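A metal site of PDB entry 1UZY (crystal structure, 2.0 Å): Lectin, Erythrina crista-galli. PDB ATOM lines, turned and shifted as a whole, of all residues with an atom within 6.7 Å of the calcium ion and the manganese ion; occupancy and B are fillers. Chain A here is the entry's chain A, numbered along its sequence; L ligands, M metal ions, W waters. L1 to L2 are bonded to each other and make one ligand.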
ATOM      1  N   ASP A  89     -24.671   4.053  16.929  1.00  0.00           N
ATOM      2  CA  ASP A  89     -23.488   4.037  17.792  1.00  0.00           C
ATOM      3  C   ASP A  89     -22.258   4.569  17.052  1.00  0.00           C
ATOM      4  O   ASP A  89     -21.293   5.003  17.681  1.00  0.00           O
ATOM      5  CB  ASP A  89     -23.170   2.622  18.270  1.00  0.00           C
ATOM      6  CG  ASP A  89     -23.842   2.281  19.590  1.00  0.00           C
ATOM      7  OD1 ASP A  89     -24.902   1.630  19.553  1.00  0.00           O
ATOM      8  OD2 ASP A  89     -23.300   2.680  20.649  1.00  0.00           O
ATOM      9  N   TYR A 106     -23.731  -2.513  18.519  1.00  0.00           N
ATOM     10  CA  TYR A 106     -23.827  -1.390  19.444  1.00  0.00           C
ATOM     11  C   TYR A 106     -22.473  -0.680  19.547  1.00  0.00           C
ATOM     12  O   TYR A 106     -21.853  -0.396  18.524  1.00  0.00           O
ATOM     13  CB  TYR A 106     -24.303  -1.881  20.819  1.00  0.00           C
ATOM     14  CG  TYR A 106     -25.594  -2.679  20.753  1.00  0.00           C
ATOM     15  CD1 TYR A 106     -25.876  -3.672  21.701  1.00  0.00           C
ATOM     16  CD2 TYR A 106     -26.522  -2.474  19.719  1.00  0.00           C
ATOM     17  CE1 TYR A 106     -27.045  -4.436  21.623  1.00  0.00           C
ATOM     18  CE2 TYR A 106     -27.690  -3.238  19.641  1.00  0.00           C
ATOM     19  CZ  TYR A 106     -27.937  -4.221  20.591  1.00  0.00           C
ATOM     20  OH  TYR A 106     -29.078  -5.002  20.512  1.00  0.00           O
ATOM     21  N   GLY A 107     -22.026  -0.412  20.765  1.00  0.00           N
ATOM     22  CA  GLY A 107     -20.763   0.275  20.986  1.00  0.00           C
ATOM     23  C   GLY A 107     -19.513  -0.428  20.479  1.00  0.00           C
ATOM     24  O   GLY A 107     -18.458   0.198  20.386  1.00  0.00           O
ATOM     25  N   TYR A 108     -19.613  -1.719  20.181  1.00  0.00           N
ATOM     26  CA  TYR A 108     -18.447  -2.455  19.677  1.00  0.00           C
ATOM     27  C   TYR A 108     -18.321  -2.263  18.163  1.00  0.00           C
ATOM     28  O   TYR A 108     -17.384  -2.758  17.529  1.00  0.00           O
ATOM     29  CB  TYR A 108     -18.539  -3.930  20.083  1.00  0.00           C
ATOM     30  CG  TYR A 108     -18.590  -4.083  21.586  1.00  0.00           C
ATOM     31  CD1 TYR A 108     -17.622  -3.488  22.395  1.00  0.00           C
ATOM     32  CD2 TYR A 108     -19.634  -4.760  22.215  1.00  0.00           C
ATOM     33  CE1 TYR A 108     -17.693  -3.545  23.781  1.00  0.00           C
ATOM     34  CE2 TYR A 108     -19.715  -4.827  23.619  1.00  0.00           C
ATOM     35  CZ  TYR A 108     -18.735  -4.219  24.397  1.00  0.00           C
ATOM     36  OH  TYR A 108     -18.805  -4.236  25.766  1.00  0.00           O
ATOM     37  N   LEU A 109     -19.285  -1.535  17.608  1.00  0.00           N
ATOM     38  CA  LEU A 109     -19.310  -1.169  16.182  1.00  0.00           C
ATOM     39  C   LEU A 109     -19.140  -2.284  15.161  1.00  0.00           C
ATOM     40  O   LEU A 109     -18.712  -2.033  14.038  1.00  0.00           O
ATOM     41  CB  LEU A 109     -18.243  -0.091  15.928  1.00  0.00           C
ATOM     42  CG  LEU A 109     -18.272   1.118  16.885  1.00  0.00           C
ATOM     43  CD1 LEU A 109     -17.143   2.084  16.546  1.00  0.00           C
ATOM     44  CD2 LEU A 109     -19.606   1.819  16.765  1.00  0.00           C
ATOM     45  N   GLU A 127     -12.278   4.954  14.465  1.00  0.00           N
ATOM     46  CA  GLU A 127     -13.704   5.089  14.689  1.00  0.00           C
ATOM     47  C   GLU A 127     -14.243   6.512  14.655  1.00  0.00           C
ATOM     48  O   GLU A 127     -13.527   7.485  14.928  1.00  0.00           O
ATOM     49  CB  GLU A 127     -14.066   4.481  16.055  1.00  0.00           C
ATOM     50  CG  GLU A 127     -13.350   5.178  17.220  1.00  0.00           C
ATOM     51  CD  GLU A 127     -13.876   4.745  18.567  1.00  0.00           C
ATOM     52  OE1 GLU A 127     -13.867   3.530  18.849  1.00  0.00           O
ATOM     53  OE2 GLU A 127     -14.293   5.624  19.354  1.00  0.00           O
ATOM     54  N   ASP A 129     -17.245   7.635  16.413  1.00  0.00           N
ATOM     55  CA  ASP A 129     -18.140   7.256  17.490  1.00  0.00           C
ATOM     56  C   ASP A 129     -19.195   8.287  17.905  1.00  0.00           C
ATOM     57  O   ASP A 129     -18.850   9.387  18.331  1.00  0.00           O
ATOM     58  CB  ASP A 129     -17.236   6.910  18.671  1.00  0.00           C
ATOM     59  CG  ASP A 129     -17.939   6.117  19.718  1.00  0.00           C
ATOM     60  OD1 ASP A 129     -19.188   6.145  19.729  1.00  0.00           O
ATOM     61  OD2 ASP A 129     -17.237   5.481  20.534  1.00  0.00           O
ATOM     62  N   THR A 130     -20.471   7.915  17.828  1.00  0.00           N
ATOM     63  CA  THR A 130     -21.587   8.817  18.145  1.00  0.00           C
ATOM     64  C   THR A 130     -22.294   8.676  19.500  1.00  0.00           C
ATOM     65  O   THR A 130     -23.127   9.515  19.849  1.00  0.00           O
ATOM     66  CB  THR A 130     -22.665   8.729  17.049  1.00  0.00           C
ATOM     67  OG1 THR A 130     -23.068   7.370  16.884  1.00  0.00           O
ATOM     68  CG2 THR A 130     -22.121   9.256  15.713  1.00  0.00           C
ATOM     69  N   PHE A 131     -21.987   7.623  20.251  1.00  0.00           N
ATOM     70  CA  PHE A 131     -22.616   7.420  21.563  1.00  0.00           C
ATOM     71  C   PHE A 131     -21.545   7.210  22.614  1.00  0.00           C
ATOM     72  O   PHE A 131     -20.632   6.429  22.419  1.00  0.00           O
ATOM     73  CB  PHE A 131     -23.518   6.179  21.539  1.00  0.00           C
ATOM     74  CG  PHE A 131     -24.206   5.902  22.846  1.00  0.00           C
ATOM     75  CD1 PHE A 131     -25.422   6.510  23.155  1.00  0.00           C
ATOM     76  CD2 PHE A 131     -23.611   5.072  23.790  1.00  0.00           C
ATOM     77  CE1 PHE A 131     -26.041   6.282  24.385  1.00  0.00           C
ATOM     78  CE2 PHE A 131     -24.225   4.846  25.029  1.00  0.00           C
ATOM     79  CZ  PHE A 131     -25.434   5.449  25.324  1.00  0.00           C
ATOM     80  N   SER A 132     -21.663   7.872  23.764  1.00  0.00           N
ATOM     81  CA  SER A 132     -20.650   7.701  24.794  1.00  0.00           C
ATOM     82  C   SER A 132     -20.905   6.511  25.721  1.00  0.00           C
ATOM     83  O   SER A 132     -21.776   6.566  26.588  1.00  0.00           O
ATOM     84  CB  SER A 132     -20.542   8.985  25.635  1.00  0.00           C
ATOM     85  OG  SER A 132     -19.518   8.871  26.595  1.00  0.00           O
ATOM     86  N   ASN A 133     -20.141   5.437  25.533  1.00  0.00           N
ATOM     87  CA  ASN A 133     -20.265   4.242  26.369  1.00  0.00           C
ATOM     88  C   ASN A 133     -19.382   4.440  27.608  1.00  0.00           C
ATOM     89  O   ASN A 133     -18.620   5.407  27.699  1.00  0.00           O
ATOM     90  CB  ASN A 133     -19.810   2.981  25.618  1.00  0.00           C
ATOM     91  CG  ASN A 133     -20.709   2.651  24.440  1.00  0.00           C
ATOM     92  OD1 ASN A 133     -20.454   3.090  23.323  1.00  0.00           O
ATOM     93  ND2 ASN A 133     -21.752   1.871  24.674  1.00  0.00           N
ATOM     94  N   TRP A 135     -16.679   3.147  28.508  1.00  0.00           N
ATOM     95  CA  TRP A 135     -15.249   3.167  28.192  1.00  0.00           C
ATOM     96  C   TRP A 135     -14.862   4.369  27.331  1.00  0.00           C
ATOM     97  O   TRP A 135     -13.692   4.515  26.984  1.00  0.00           O
ATOM     98  CB  TRP A 135     -14.873   1.888  27.450  1.00  0.00           C
ATOM     99  CG  TRP A 135     -15.681   1.697  26.182  1.00  0.00           C
ATOM    100  CD1 TRP A 135     -15.486   2.308  24.982  1.00  0.00           C
ATOM    101  CD2 TRP A 135     -16.833   0.850  26.028  1.00  0.00           C
ATOM    102  NE1 TRP A 135     -16.447   1.905  24.085  1.00  0.00           N
ATOM    103  CE2 TRP A 135     -17.285   1.003  24.695  1.00  0.00           C
ATOM    104  CE3 TRP A 135     -17.524  -0.028  26.876  1.00  0.00           C
ATOM    105  CZ2 TRP A 135     -18.391   0.328  24.197  1.00  0.00           C
ATOM    106  CZ3 TRP A 135     -18.638  -0.708  26.383  1.00  0.00           C
ATOM    107  CH2 TRP A 135     -19.052  -0.531  25.050  1.00  0.00           C
ATOM    108  N   ASP A 136     -15.837   5.206  26.981  1.00  0.00           N
ATOM    109  CA  ASP A 136     -15.607   6.377  26.126  1.00  0.00           C
ATOM    110  C   ASP A 136     -15.440   7.702  26.840  1.00  0.00           C
ATOM    111  O   ASP A 136     -15.816   7.853  28.004  1.00  0.00           O
ATOM    112  CB  ASP A 136     -16.812   6.622  25.197  1.00  0.00           C
ATOM    113  CG  ASP A 136     -16.861   5.684  24.026  1.00  0.00           C
ATOM    114  OD1 ASP A 136     -15.814   5.413  23.416  1.00  0.00           O
ATOM    115  OD2 ASP A 136     -17.979   5.240  23.728  1.00  0.00           O
ATOM    116  N   PRO A 137     -14.873   8.689  26.132  1.00  0.00           N
ATOM    117  CA  PRO A 137     -14.714  10.007  26.737  1.00  0.00           C
ATOM    118  C   PRO A 137     -16.170  10.487  26.712  1.00  0.00           C
ATOM    119  O   PRO A 137     -16.986   9.931  25.966  1.00  0.00           O
ATOM    120  CB  PRO A 137     -13.823  10.743  25.736  1.00  0.00           C
ATOM    121  CG  PRO A 137     -14.137  10.084  24.424  1.00  0.00           C
ATOM    122  CD  PRO A 137     -14.165   8.624  24.839  1.00  0.00           C
ATOM    123  N   VAL A 140     -19.206  13.370  22.407  1.00  0.00           N
ATOM    124  CA  VAL A 140     -19.587  12.659  21.194  1.00  0.00           C
ATOM    125  C   VAL A 140     -20.235  13.652  20.232  1.00  0.00           C
ATOM    126  O   VAL A 140     -20.936  14.576  20.648  1.00  0.00           O
ATOM    127  CB  VAL A 140     -20.603  11.504  21.456  1.00  0.00           C
ATOM    128  CG1 VAL A 140     -19.893  10.308  22.063  1.00  0.00           C
ATOM    129  CG2 VAL A 140     -21.708  11.990  22.373  1.00  0.00           C
ATOM    130  N   HIS A 142     -16.885  11.592  18.425  1.00  0.00           N
ATOM    131  CA  HIS A 142     -15.444  11.713  18.543  1.00  0.00           C
ATOM    132  C   HIS A 142     -14.771  10.713  17.629  1.00  0.00           C
ATOM    133  O   HIS A 142     -15.314   9.624  17.351  1.00  0.00           O
ATOM    134  CB  HIS A 142     -14.964  11.495  19.995  1.00  0.00           C
ATOM    135  CG  HIS A 142     -15.294  10.146  20.563  1.00  0.00           C
ATOM    136  ND1 HIS A 142     -16.346   9.938  21.425  1.00  0.00           N
ATOM    137  CD2 HIS A 142     -14.688   8.937  20.407  1.00  0.00           C
ATOM    138  CE1 HIS A 142     -16.384   8.665  21.785  1.00  0.00           C
ATOM    139  NE2 HIS A 142     -15.386   8.036  21.172  1.00  0.00           N
ATOM    140  N   ILE A 143     -13.599  11.100  17.112  1.00  0.00           N
ATOM    141  CA  ILE A 143     -12.816  10.218  16.271  1.00  0.00           C
ATOM    142  C   ILE A 143     -11.966   9.448  17.268  1.00  0.00           C
ATOM    143  O   ILE A 143     -11.605   9.984  18.322  1.00  0.00           O
ATOM    144  CB  ILE A 143     -11.847  10.990  15.350  1.00  0.00           C
ATOM    145  CG1 ILE A 143     -12.582  12.091  14.587  1.00  0.00           C
ATOM    146  CG2 ILE A 143     -11.181  10.008  14.380  1.00  0.00           C
ATOM    147  CD1 ILE A 143     -11.665  12.952  13.714  1.00  0.00           C
ATOM    148  N   GLY A 144     -11.656   8.199  16.953  1.00  0.00           N
ATOM    149  CA  GLY A 144     -10.846   7.409  17.860  1.00  0.00           C
ATOM    150  C   GLY A 144      -9.918   6.453  17.136  1.00  0.00           C
ATOM    151  O   GLY A 144     -10.270   5.897  16.092  1.00  0.00           O
ATOM    152  N   ASP A 146      -8.249   3.024  17.503  1.00  0.00           N
ATOM    153  CA  ASP A 146      -8.385   1.797  18.283  1.00  0.00           C
ATOM    154  C   ASP A 146      -7.355   0.740  17.907  1.00  0.00           C
ATOM    155  O   ASP A 146      -7.221   0.370  16.742  1.00  0.00           O
ATOM    156  CB  ASP A 146      -9.780   1.198  18.095  1.00  0.00           C
ATOM    157  CG  ASP A 146     -10.903   2.184  18.392  1.00  0.00           C
ATOM    158  OD1 ASP A 146     -10.651   3.208  19.071  1.00  0.00           O
ATOM    159  OD2 ASP A 146     -12.038   1.929  17.941  1.00  0.00           O
ATOM    160  N   ILE A 150     -11.729  -1.499  21.904  1.00  0.00           N
ATOM    161  CA  ILE A 150     -12.693  -0.458  21.600  1.00  0.00           C
ATOM    162  C   ILE A 150     -12.351   0.755  22.476  1.00  0.00           C
ATOM    163  O   ILE A 150     -12.884   1.849  22.292  1.00  0.00           O
ATOM    164  CB  ILE A 150     -14.135  -0.917  21.894  1.00  0.00           C
ATOM    165  CG1 ILE A 150     -15.133   0.091  21.339  1.00  0.00           C
ATOM    166  CG2 ILE A 150     -14.325  -1.125  23.398  1.00  0.00           C
ATOM    167  CD1 ILE A 150     -15.130   0.193  19.811  1.00  0.00           C
ATOM    168  N   ARG A 151     -11.467   0.535  23.445  1.00  0.00           N
ATOM    169  CA  ARG A 151     -11.003   1.597  24.325  1.00  0.00           C
ATOM    170  C   ARG A 151      -9.868   2.298  23.577  1.00  0.00           C
ATOM    171  O   ARG A 151      -8.708   1.902  23.665  1.00  0.00           O
ATOM    172  CB  ARG A 151     -10.500   1.008  25.647  1.00  0.00           C
ATOM    173  CG  ARG A 151     -11.578   0.327  26.488  1.00  0.00           C
ATOM    174  CD  ARG A 151     -11.005  -0.271  27.774  1.00  0.00           C
ATOM    175  NE  ARG A 151     -12.019  -1.034  28.502  1.00  0.00           N
ATOM    176  CZ  ARG A 151     -12.878  -0.525  29.389  1.00  0.00           C
ATOM    177  NH1 ARG A 151     -12.863   0.774  29.675  1.00  0.00           N
ATOM    178  NH2 ARG A 151     -13.770  -1.311  29.966  1.00  0.00           N
ATOM    179  N   SER A 152     -10.214   3.345  22.847  1.00  0.00           N
ATOM    180  CA  SER A 152      -9.264   4.106  22.039  1.00  0.00           C
ATOM    181  C   SER A 152      -7.989   4.544  22.756  1.00  0.00           C
ATOM    182  O   SER A 152      -8.028   4.980  23.908  1.00  0.00           O
ATOM    183  CB  SER A 152      -9.952   5.367  21.480  1.00  0.00           C
ATOM    184  OG  SER A 152     -11.169   5.038  20.831  1.00  0.00           O
ATOM    185  N   THR A 155      -8.407   9.902  21.281  1.00  0.00           N
ATOM    186  CA  THR A 155      -9.692  10.353  20.750  1.00  0.00           C
ATOM    187  C   THR A 155      -9.672  11.851  20.481  1.00  0.00           C
ATOM    188  O   THR A 155      -8.878  12.595  21.064  1.00  0.00           O
ATOM    189  CB  THR A 155     -10.873  10.051  21.716  1.00  0.00           C
ATOM    190  OG1 THR A 155     -10.655  10.709  22.964  1.00  0.00           O
ATOM    191  CG2 THR A 155     -11.022   8.538  21.940  1.00  0.00           C
HETATM  192  C1  LIG L   1     -30.625   0.073  27.532  1.00  0.00           C
HETATM  193  C2  LIG L   1     -29.704  -0.151  26.334  1.00  0.00           C
HETATM  194  C3  LIG L   1     -28.243   0.001  26.789  1.00  0.00           C
HETATM  195  C4  LIG L   1     -27.960  -1.045  27.916  1.00  0.00           C
HETATM  196  C5  LIG L   1     -26.546  -0.928  28.457  1.00  0.00           C
HETATM  197  C6  LIG L   1     -30.294  -0.982  28.612  1.00  0.00           C
HETATM  198  O1  LIG L   1     -31.108  -0.791  29.714  1.00  0.00           O
HETATM  199  O2  LIG L   1     -31.982  -0.082  27.125  1.00  0.00           O
HETATM  200  O3  LIG L   1     -29.990   0.820  25.333  1.00  0.00           O
HETATM  201  O4  LIG L   1     -27.347  -0.217  25.671  1.00  0.00           O
HETATM  202  O5  LIG L   1     -28.894  -0.851  29.034  1.00  0.00           O
HETATM  203  O6  LIG L   1     -26.280  -1.950  29.407  1.00  0.00           O
HETATM  204  C1  LG2 L   2     -26.744   0.904  25.073  1.00  0.00           C
HETATM  205  C2  LG2 L   2     -25.574   0.418  24.190  1.00  0.00           C
HETATM  206  C3  LG2 L   2     -24.893   1.630  23.515  1.00  0.00           C
HETATM  207  C4  LG2 L   2     -25.927   2.388  22.640  1.00  0.00           C
HETATM  208  C5  LG2 L   2     -27.092   2.802  23.598  1.00  0.00           C
HETATM  209  C6  LG2 L   2     -28.226   3.552  22.980  1.00  0.00           C
HETATM  210  O1  LG2 L   2     -24.643  -0.275  25.008  1.00  0.00           O
HETATM  211  O2  LG2 L   2     -23.819   1.186  22.712  1.00  0.00           O
HETATM  212  O3  LG2 L   2     -26.409   1.525  21.616  1.00  0.00           O
HETATM  213  O4  LG2 L   2     -27.666   1.629  24.245  1.00  0.00           O
HETATM  214  O5  LG2 L   2     -29.192   3.834  23.978  1.00  0.00           O
HETATM  215 CA    CA M   1     -19.231   4.512  21.745  1.00  0.00          CA
HETATM  216 MN    MN M   2     -15.242   5.678  21.307  1.00  0.00          MN
HETATM  217  O   HOH W   1     -14.855   3.387  21.237  1.00  0.00           O
HETATM  218  O   HOH W   2     -21.020   3.781  20.076  1.00  0.00           O
HETATM  219  O   HOH W   3     -17.681   2.565  21.225  1.00  0.00           O
HETATM  220  O   HOH W   4     -13.250   5.914  22.235  1.00  0.00           O
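The manganese ion is bound by the side-chain carboxylate (OD2) of Asp 129 (2.1 Å), the side-chain carboxylate (OE2) of Glu 127 (2.2 Å), the side-chain carboxylate (OD1) of Asp 136 (2.2 Å), water W4 (2.2 Å), water W1 (2.3 Å) and a ring nitrogen (NE2) of His 142 (2.4 Å).
Within 4 Å of the calcium ion: Asp 129, Phe 131, Asn 133 and Asp 136.
The nearest printed residue that does not touch the calcium ion is Trp 135 (4.5 Å).
ND2 of Asn 133 sits at hydrogen-bond distance from O2 of LG2 L2 (2.9 Å).
The backbone NH (N) of Gly 107 lies within hydrogen-bond range of an oxygen (O2) of LG2 L2, 3.1 Å away.
An oxygen (O3) of LG2 L2 sits at hydrogen-bond distance from the side-chain carboxylate (OD1) of Asp 89, at 2.6 Å.
The calcium ion is bound by OD1 of Asn 133 (2.5 Å), OD2 of Asp 136 (2.5 Å), O of Phe 131 (2.5 Å), OD2 of Asp 129 (2.5 Å), water W3 (2.5 Å), water W2 (2.6 Å) and OD1 of Asp 129 (2.6 Å).
The calcium ion has seven donor atoms within binding distance.
Water W3 lies within hydrogen-bond range of O of Gly 107 (2.6 Å) and NE1 of Trp 135 (3.2 Å).
Water W1 lies within hydrogen-bond range of the side-chain carboxylate (OE1) of Glu 127 (2.6 Å) and the backbone carbonyl oxygen (O) of Ile 150 (2.7 Å).
The side-chain carboxylate (OE1) of Glu 127 lies close to the side-chain carboxylate (OD2) of Asp 146.
N of Glu 127 lies within hydrogen-bond range of O of Gly 144, at 2.8 Å.
Four residues have an atom within 4 Å of the manganese ion: Glu 127, Asp 129, Asp 136 and His 142.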
